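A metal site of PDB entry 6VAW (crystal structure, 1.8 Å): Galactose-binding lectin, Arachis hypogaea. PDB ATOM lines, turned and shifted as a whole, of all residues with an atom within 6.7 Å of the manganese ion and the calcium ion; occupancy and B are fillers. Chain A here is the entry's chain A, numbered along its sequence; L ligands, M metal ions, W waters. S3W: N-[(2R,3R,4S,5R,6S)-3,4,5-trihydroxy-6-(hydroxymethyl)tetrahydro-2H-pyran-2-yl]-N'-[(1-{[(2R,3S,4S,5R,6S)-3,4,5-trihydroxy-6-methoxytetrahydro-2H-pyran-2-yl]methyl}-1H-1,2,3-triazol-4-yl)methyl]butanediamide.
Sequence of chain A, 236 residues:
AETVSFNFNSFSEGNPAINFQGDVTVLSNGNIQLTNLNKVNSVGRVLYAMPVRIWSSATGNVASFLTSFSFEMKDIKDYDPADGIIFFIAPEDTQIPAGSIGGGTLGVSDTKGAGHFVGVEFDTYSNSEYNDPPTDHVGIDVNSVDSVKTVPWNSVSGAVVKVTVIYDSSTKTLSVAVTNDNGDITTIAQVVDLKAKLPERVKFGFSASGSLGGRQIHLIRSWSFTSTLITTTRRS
The side-chain carboxylate (OD1) of Asp 83 lies within hydrogen-bond range of an oxygen (O4) of the ligand (2.6 Å).
An oxygen (O3) of the ligand is in hydrogen-bond range of the backbone NH of Gly 104, 3.0 Å away.
ND2 of Asn 127 is in hydrogen-bond range of O3 of the ligand, at 2.8 Å.
OG of Ser 126 lies within hydrogen-bond range of O of Asp 132 (3.5 Å).
OE1 of Glu 121 sits close to OD2 of Asp 141 (2.7 Å).
The backbone NH (N) of Glu 121 is in hydrogen-bond range of the backbone carbonyl oxygen (O) of Gly 139 (2.9 Å).
Of the 23 residues printed, 4 come within 4 Å of the manganese ion.
Along chain A the residues within 4 Å of the manganese ion span positions 121 to 137.
Of the 23 residues printed, 4 come within 4 Å of the calcium ion.
The nearest printed residue that does not touch the calcium ion is Ser 126 (4.3 Å).
The manganese ion is bound by OD2 of Asp 123, NE2 of His 137, OE2 of Glu 121, OD1 of Asp 132, water W1 and water W2.
The calcium ion is bound by the backbone carbonyl oxygen (O) of Tyr 125 (2.1 Å), water W3 (2.3 Å), the side-chain carboxylate (OD2) of Asp 132 (2.4 Å), water W4 (2.4 Å), the side-chain amide oxygen (OD1) of Asn 127 (2.5 Å), the side-chain carboxylate (OD1) of Asp 123 (2.5 Å) and the side-chain carboxylate (OD2) of Asp 123 (2.6 Å).
Water W2 bridges O of Val 145 (2.6 Å) and OE1 of Glu 121 (2.7 Å).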
ATOM      1  N   ASP A  83     -13.110 -21.094  26.382  1.00  0.00           N
ATOM      2  CA  ASP A  83     -12.392 -21.734  25.272  1.00  0.00           C
ATOM      3  C   ASP A  83     -13.148 -21.829  23.933  1.00  0.00           C
ATOM      4  O   ASP A  83     -12.511 -22.160  22.931  1.00  0.00           O
ATOM      5  CB  ASP A  83     -11.971 -23.117  25.674  1.00  0.00           C
ATOM      6  CG  ASP A  83     -10.682 -23.071  26.434  1.00  0.00           C
ATOM      7  OD1 ASP A  83     -10.737 -22.887  27.680  1.00  0.00           O
ATOM      8  OD2 ASP A  83      -9.613 -23.092  25.786  1.00  0.00           O
ATOM      9  N   GLY A 103     -11.482 -26.599  29.485  1.00  0.00           N
ATOM     10  CA  GLY A 103     -10.479 -25.973  28.632  1.00  0.00           C
ATOM     11  C   GLY A 103     -10.646 -26.274  27.151  1.00  0.00           C
ATOM     12  O   GLY A 103     -11.750 -26.139  26.604  1.00  0.00           O
ATOM     13  N   GLY A 104      -9.562 -26.702  26.512  1.00  0.00           N
ATOM     14  CA  GLY A 104      -9.480 -27.022  25.092  1.00  0.00           C
ATOM     15  C   GLY A 104     -10.267 -28.262  24.678  1.00  0.00           C
ATOM     16  O   GLY A 104     -10.421 -28.508  23.478  1.00  0.00           O
ATOM     17  N   THR A 105     -10.707 -29.071  25.666  1.00  0.00           N
ATOM     18  CA  THR A 105     -11.490 -30.281  25.419  1.00  0.00           C
ATOM     19  C   THR A 105     -12.921 -29.931  24.961  1.00  0.00           C
ATOM     20  O   THR A 105     -13.640 -30.830  24.536  1.00  0.00           O
ATOM     21  CB  THR A 105     -11.528 -31.231  26.652  1.00  0.00           C
ATOM     22  OG1 THR A 105     -12.489 -30.763  27.627  1.00  0.00           O
ATOM     23  CG2 THR A 105     -10.173 -31.497  27.258  1.00  0.00           C
ATOM     24  N   LEU A 106     -13.365 -28.664  25.197  1.00  0.00           N
ATOM     25  CA  LEU A 106     -14.691 -28.076  24.871  1.00  0.00           C
ATOM     26  C   LEU A 106     -15.874 -28.861  25.512  1.00  0.00           C
ATOM     27  O   LEU A 106     -17.028 -28.712  25.071  1.00  0.00           O
ATOM     28  CB  LEU A 106     -14.866 -27.952  23.328  1.00  0.00           C
ATOM     29  CG  LEU A 106     -13.811 -27.124  22.593  1.00  0.00           C
ATOM     30  CD1 LEU A 106     -13.983 -27.245  21.064  1.00  0.00           C
ATOM     31  CD2 LEU A 106     -13.806 -25.649  23.060  1.00  0.00           C
ATOM     32  N   GLU A 121     -16.810 -26.836  15.850  1.00  0.00           N
ATOM     33  CA  GLU A 121     -16.288 -26.006  16.942  1.00  0.00           C
ATOM     34  C   GLU A 121     -16.023 -24.581  16.500  1.00  0.00           C
ATOM     35  O   GLU A 121     -15.598 -24.320  15.369  1.00  0.00           O
ATOM     36  CB  GLU A 121     -15.010 -26.590  17.551  1.00  0.00           C
ATOM     37  CG  GLU A 121     -13.901 -26.781  16.518  1.00  0.00           C
ATOM     38  CD  GLU A 121     -12.576 -27.094  17.158  1.00  0.00           C
ATOM     39  OE1 GLU A 121     -12.489 -28.167  17.777  1.00  0.00           O
ATOM     40  OE2 GLU A 121     -11.622 -26.306  17.006  1.00  0.00           O
ATOM     41  N   ASP A 123     -13.743 -22.219  18.087  1.00  0.00           N
ATOM     42  CA  ASP A 123     -12.600 -22.279  18.986  1.00  0.00           C
ATOM     43  C   ASP A 123     -11.876 -20.950  19.116  1.00  0.00           C
ATOM     44  O   ASP A 123     -11.404 -20.391  18.133  1.00  0.00           O
ATOM     45  CB  ASP A 123     -11.670 -23.369  18.472  1.00  0.00           C
ATOM     46  CG  ASP A 123     -10.692 -23.851  19.492  1.00  0.00           C
ATOM     47  OD1 ASP A 123     -10.602 -23.223  20.574  1.00  0.00           O
ATOM     48  OD2 ASP A 123     -10.048 -24.879  19.248  1.00  0.00           O
ATOM     49  N   THR A 124     -11.795 -20.437  20.368  1.00  0.00           N
ATOM     50  CA  THR A 124     -11.228 -19.117  20.646  1.00  0.00           C
ATOM     51  C   THR A 124      -9.867 -19.157  21.382  1.00  0.00           C
ATOM     52  O   THR A 124      -9.361 -18.101  21.784  1.00  0.00           O
ATOM     53  CB  THR A 124     -12.235 -18.258  21.420  1.00  0.00           C
ATOM     54  OG1 THR A 124     -12.415 -18.774  22.735  1.00  0.00           O
ATOM     55  CG2 THR A 124     -13.585 -18.160  20.722  1.00  0.00           C
ATOM     56  N   TYR A 125      -9.237 -20.351  21.494  1.00  0.00           N
ATOM     57  CA  TYR A 125      -7.928 -20.503  22.162  1.00  0.00           C
ATOM     58  C   TYR A 125      -7.127 -21.616  21.485  1.00  0.00           C
ATOM     59  O   TYR A 125      -7.631 -22.728  21.290  1.00  0.00           O
ATOM     60  CB  TYR A 125      -8.095 -20.764  23.675  1.00  0.00           C
ATOM     61  CG  TYR A 125      -6.752 -20.807  24.388  1.00  0.00           C
ATOM     62  CD1 TYR A 125      -6.000 -21.985  24.439  1.00  0.00           C
ATOM     63  CD2 TYR A 125      -6.208 -19.665  24.966  1.00  0.00           C
ATOM     64  CE1 TYR A 125      -4.732 -22.009  25.006  1.00  0.00           C
ATOM     65  CE2 TYR A 125      -4.965 -19.689  25.588  1.00  0.00           C
ATOM     66  CZ  TYR A 125      -4.231 -20.869  25.615  1.00  0.00           C
ATOM     67  OH  TYR A 125      -3.010 -20.898  26.238  1.00  0.00           O
ATOM     68  N   SER A 126      -5.860 -21.330  21.159  1.00  0.00           N
ATOM     69  CA  SER A 126      -4.978 -22.272  20.474  1.00  0.00           C
ATOM     70  C   SER A 126      -4.277 -23.214  21.449  1.00  0.00           C
ATOM     71  O   SER A 126      -3.357 -22.807  22.148  1.00  0.00           O
ATOM     72  CB  SER A 126      -3.951 -21.524  19.628  1.00  0.00           C
ATOM     73  OG  SER A 126      -3.154 -22.419  18.881  1.00  0.00           O
ATOM     74  N   ASN A 127      -4.742 -24.480  21.497  1.00  0.00           N
ATOM     75  CA  ASN A 127      -4.188 -25.531  22.338  1.00  0.00           C
ATOM     76  C   ASN A 127      -3.198 -26.321  21.504  1.00  0.00           C
ATOM     77  O   ASN A 127      -3.601 -27.075  20.614  1.00  0.00           O
ATOM     78  CB  ASN A 127      -5.291 -26.425  22.888  1.00  0.00           C
ATOM     79  CG  ASN A 127      -6.261 -25.702  23.758  1.00  0.00           C
ATOM     80  OD1 ASN A 127      -7.139 -24.970  23.287  1.00  0.00           O
ATOM     81  ND2 ASN A 127      -6.100 -25.829  25.056  1.00  0.00           N
ATOM     82  N   TYR A 130      -3.554 -30.072  21.114  1.00  0.00           N
ATOM     83  CA  TYR A 130      -4.616 -30.536  20.193  1.00  0.00           C
ATOM     84  C   TYR A 130      -4.384 -30.072  18.772  1.00  0.00           C
ATOM     85  O   TYR A 130      -5.308 -30.119  17.954  1.00  0.00           O
ATOM     86  CB  TYR A 130      -5.990 -30.063  20.696  1.00  0.00           C
ATOM     87  CG  TYR A 130      -6.281 -30.493  22.116  1.00  0.00           C
ATOM     88  CD1 TYR A 130      -6.057 -31.809  22.528  1.00  0.00           C
ATOM     89  CD2 TYR A 130      -6.835 -29.608  23.032  1.00  0.00           C
ATOM     90  CE1 TYR A 130      -6.326 -32.209  23.829  1.00  0.00           C
ATOM     91  CE2 TYR A 130      -7.075 -29.992  24.350  1.00  0.00           C
ATOM     92  CZ  TYR A 130      -6.821 -31.300  24.750  1.00  0.00           C
ATOM     93  OH  TYR A 130      -7.079 -31.714  26.027  1.00  0.00           O
ATOM     94  N   ASN A 131      -3.153 -29.636  18.483  1.00  0.00           N
ATOM     95  CA  ASN A 131      -2.659 -29.146  17.202  1.00  0.00           C
ATOM     96  C   ASN A 131      -3.572 -28.043  16.613  1.00  0.00           C
ATOM     97  O   ASN A 131      -3.820 -28.026  15.404  1.00  0.00           O
ATOM     98  CB  ASN A 131      -2.447 -30.306  16.198  1.00  0.00           C
ATOM     99  CG  ASN A 131      -1.327 -31.238  16.607  1.00  0.00           C
ATOM    100  OD1 ASN A 131      -0.193 -30.822  16.865  1.00  0.00           O
ATOM    101  ND2 ASN A 131      -1.611 -32.533  16.674  1.00  0.00           N
ATOM    102  N   ASP A 132      -4.040 -27.121  17.477  1.00  0.00           N
ATOM    103  CA  ASP A 132      -4.901 -26.015  17.051  1.00  0.00           C
ATOM    104  C   ASP A 132      -4.153 -25.074  16.121  1.00  0.00           C
ATOM    105  O   ASP A 132      -2.979 -24.825  16.367  1.00  0.00           O
ATOM    106  CB  ASP A 132      -5.397 -25.215  18.267  1.00  0.00           C
ATOM    107  CG  ASP A 132      -6.717 -25.674  18.864  1.00  0.00           C
ATOM    108  OD1 ASP A 132      -7.517 -26.300  18.127  1.00  0.00           O
ATOM    109  OD2 ASP A 132      -6.953 -25.402  20.058  1.00  0.00           O
ATOM    110  N   PRO A 133      -4.831 -24.451  15.130  1.00  0.00           N
ATOM    111  CA  PRO A 133      -4.137 -23.426  14.318  1.00  0.00           C
ATOM    112  C   PRO A 133      -3.813 -22.186  15.189  1.00  0.00           C
ATOM    113  O   PRO A 133      -4.352 -22.077  16.291  1.00  0.00           O
ATOM    114  CB  PRO A 133      -5.123 -23.124  13.174  1.00  0.00           C
ATOM    115  CG  PRO A 133      -6.446 -23.561  13.677  1.00  0.00           C
ATOM    116  CD  PRO A 133      -6.245 -24.617  14.717  1.00  0.00           C
ATOM    117  N   HIS A 137     -10.749 -20.113  15.148  1.00  0.00           N
ATOM    118  CA  HIS A 137     -11.087 -20.920  13.987  1.00  0.00           C
ATOM    119  C   HIS A 137     -12.387 -21.672  14.169  1.00  0.00           C
ATOM    120  O   HIS A 137     -12.837 -21.900  15.303  1.00  0.00           O
ATOM    121  CB  HIS A 137      -9.955 -21.944  13.703  1.00  0.00           C
ATOM    122  CG  HIS A 137      -9.594 -22.781  14.890  1.00  0.00           C
ATOM    123  ND1 HIS A 137      -8.747 -22.303  15.897  1.00  0.00           N
ATOM    124  CD2 HIS A 137      -9.938 -24.052  15.194  1.00  0.00           C
ATOM    125  CE1 HIS A 137      -8.637 -23.284  16.772  1.00  0.00           C
ATOM    126  NE2 HIS A 137      -9.330 -24.359  16.393  1.00  0.00           N
ATOM    127  N   VAL A 138     -12.954 -22.091  13.038  1.00  0.00           N
ATOM    128  CA  VAL A 138     -14.100 -22.986  12.980  1.00  0.00           C
ATOM    129  C   VAL A 138     -13.515 -24.305  12.545  1.00  0.00           C
ATOM    130  O   VAL A 138     -12.695 -24.346  11.622  1.00  0.00           O
ATOM    131  CB  VAL A 138     -15.254 -22.497  12.073  1.00  0.00           C
ATOM    132  CG1 VAL A 138     -16.437 -23.475  12.111  1.00  0.00           C
ATOM    133  CG2 VAL A 138     -15.720 -21.097  12.466  1.00  0.00           C
ATOM    134  N   GLY A 139     -13.877 -25.382  13.222  1.00  0.00           N
ATOM    135  CA  GLY A 139     -13.340 -26.693  12.901  1.00  0.00           C
ATOM    136  C   GLY A 139     -14.393 -27.749  12.788  1.00  0.00           C
ATOM    137  O   GLY A 139     -15.465 -27.620  13.364  1.00  0.00           O
ATOM    138  N   ASP A 141     -14.895 -31.642  13.608  1.00  0.00           N
ATOM    139  CA  ASP A 141     -14.326 -32.640  14.532  1.00  0.00           C
ATOM    140  C   ASP A 141     -14.980 -33.971  14.423  1.00  0.00           C
ATOM    141  O   ASP A 141     -16.184 -34.071  14.472  1.00  0.00           O
ATOM    142  CB  ASP A 141     -14.512 -32.172  15.976  1.00  0.00           C
ATOM    143  CG  ASP A 141     -13.741 -30.934  16.343  1.00  0.00           C
ATOM    144  OD1 ASP A 141     -12.896 -30.499  15.535  1.00  0.00           O
ATOM    145  OD2 ASP A 141     -13.918 -30.457  17.470  1.00  0.00           O
ATOM    146  N   VAL A 145     -10.879 -33.344  19.313  1.00  0.00           N
ATOM    147  CA  VAL A 145     -10.776 -31.889  19.255  1.00  0.00           C
ATOM    148  C   VAL A 145      -9.497 -31.510  18.474  1.00  0.00           C
ATOM    149  O   VAL A 145      -9.153 -30.328  18.354  1.00  0.00           O
ATOM    150  CB  VAL A 145     -10.884 -31.160  20.631  1.00  0.00           C
ATOM    151  CG1 VAL A 145     -12.299 -31.267  21.195  1.00  0.00           C
ATOM    152  CG2 VAL A 145      -9.854 -31.673  21.631  1.00  0.00           C
ATOM    153  N   ASP A 146      -8.793 -32.517  17.902  1.00  0.00           N
ATOM    154  CA  ASP A 146      -7.729 -32.322  16.911  1.00  0.00           C
ATOM    155  C   ASP A 146      -8.504 -32.414  15.578  1.00  0.00           C
ATOM    156  O   ASP A 146      -8.734 -33.498  15.055  1.00  0.00           O
ATOM    157  CB  ASP A 146      -6.593 -33.360  17.023  1.00  0.00           C
ATOM    158  CG  ASP A 146      -5.390 -33.074  16.118  1.00  0.00           C
ATOM    159  OD1 ASP A 146      -5.571 -32.410  15.061  1.00  0.00           O
ATOM    160  OD2 ASP A 146      -4.265 -33.511  16.463  1.00  0.00           O
ATOM    161  N   SER A 147      -9.017 -31.273  15.124  1.00  0.00           N
ATOM    162  CA  SER A 147      -9.936 -31.211  13.987  1.00  0.00           C
ATOM    163  C   SER A 147      -9.428 -31.869  12.695  1.00  0.00           C
ATOM    164  O   SER A 147      -8.252 -31.800  12.335  1.00  0.00           O
ATOM    165  CB  SER A 147     -10.327 -29.778  13.688  1.00  0.00           C
ATOM    166  OG  SER A 147     -10.794 -29.125  14.845  1.00  0.00           O
ATOM    167  N   THR A 150      -9.951 -27.185   9.613  1.00  0.00           N
ATOM    168  CA  THR A 150     -10.239 -25.893  10.231  1.00  0.00           C
ATOM    169  C   THR A 150     -10.194 -24.795   9.174  1.00  0.00           C
ATOM    170  O   THR A 150      -9.579 -24.955   8.108  1.00  0.00           O
ATOM    171  CB  THR A 150      -9.280 -25.500  11.406  1.00  0.00           C
ATOM    172  OG1 THR A 150      -7.977 -25.243  10.905  1.00  0.00           O
ATOM    173  CG2 THR A 150      -9.269 -26.503  12.555  1.00  0.00           C
HETATM  174  N1  S3W L   1      -4.432 -24.033  30.640  1.00  0.00           N
HETATM  175  N2  S3W L   1      -1.849 -21.812  34.595  1.00  0.00           N
HETATM  176  C11 S3W L   1      -2.377 -20.816  35.497  1.00  0.00           C
HETATM  177  C4  S3W L   1      -7.164 -22.228  27.951  1.00  0.00           C
HETATM  178  C3  S3W L   1      -6.617 -23.612  27.603  1.00  0.00           C
HETATM  179  C5  S3W L   1      -6.102 -21.435  28.719  1.00  0.00           C
HETATM  180  C1  S3W L   1      -4.984 -23.411  29.476  1.00  0.00           C
HETATM  181  C2  S3W L   1      -6.053 -24.298  28.843  1.00  0.00           C
HETATM  182  C6  S3W L   1      -6.328 -19.989  29.074  1.00  0.00           C
HETATM  183  C7  S3W L   1      -3.184 -23.815  31.071  1.00  0.00           C
HETATM  184  C8  S3W L   1      -2.766 -24.590  32.302  1.00  0.00           C
HETATM  185  C9  S3W L   1      -1.855 -23.807  33.238  1.00  0.00           C
HETATM  186  C10 S3W L   1      -2.590 -22.795  34.079  1.00  0.00           C
HETATM  187  O5  S3W L   1      -5.558 -22.152  29.842  1.00  0.00           O
HETATM  188  O2  S3W L   1      -5.485 -25.547  28.484  1.00  0.00           O
HETATM  189  O3  S3W L   1      -7.612 -24.415  26.989  1.00  0.00           O
HETATM  190  O4  S3W L   1      -8.364 -22.346  28.701  1.00  0.00           O
HETATM  191  O6  S3W L   1      -5.093 -19.276  29.112  1.00  0.00           O
HETATM  192  O10 S3W L   1      -3.795 -22.901  34.296  1.00  0.00           O
HETATM  193  O7  S3W L   1      -2.403 -23.068  30.492  1.00  0.00           O
HETATM  194 MN    MN M   1      -9.605 -26.041  17.594  1.00  0.00          MN
HETATM  195 CA    CA M   2      -8.708 -24.579  21.418  1.00  0.00          CA
HETATM  196  O   HOH W   1      -8.963 -27.356  15.846  1.00  0.00           O
HETATM  197  O   HOH W   2     -10.116 -28.000  19.043  1.00  0.00           O
HETATM  198  O   HOH W   3     -10.099 -23.936  23.125  1.00  0.00           O
HETATM  199  O   HOH W   4      -9.463 -26.856  21.559  1.00  0.00           O
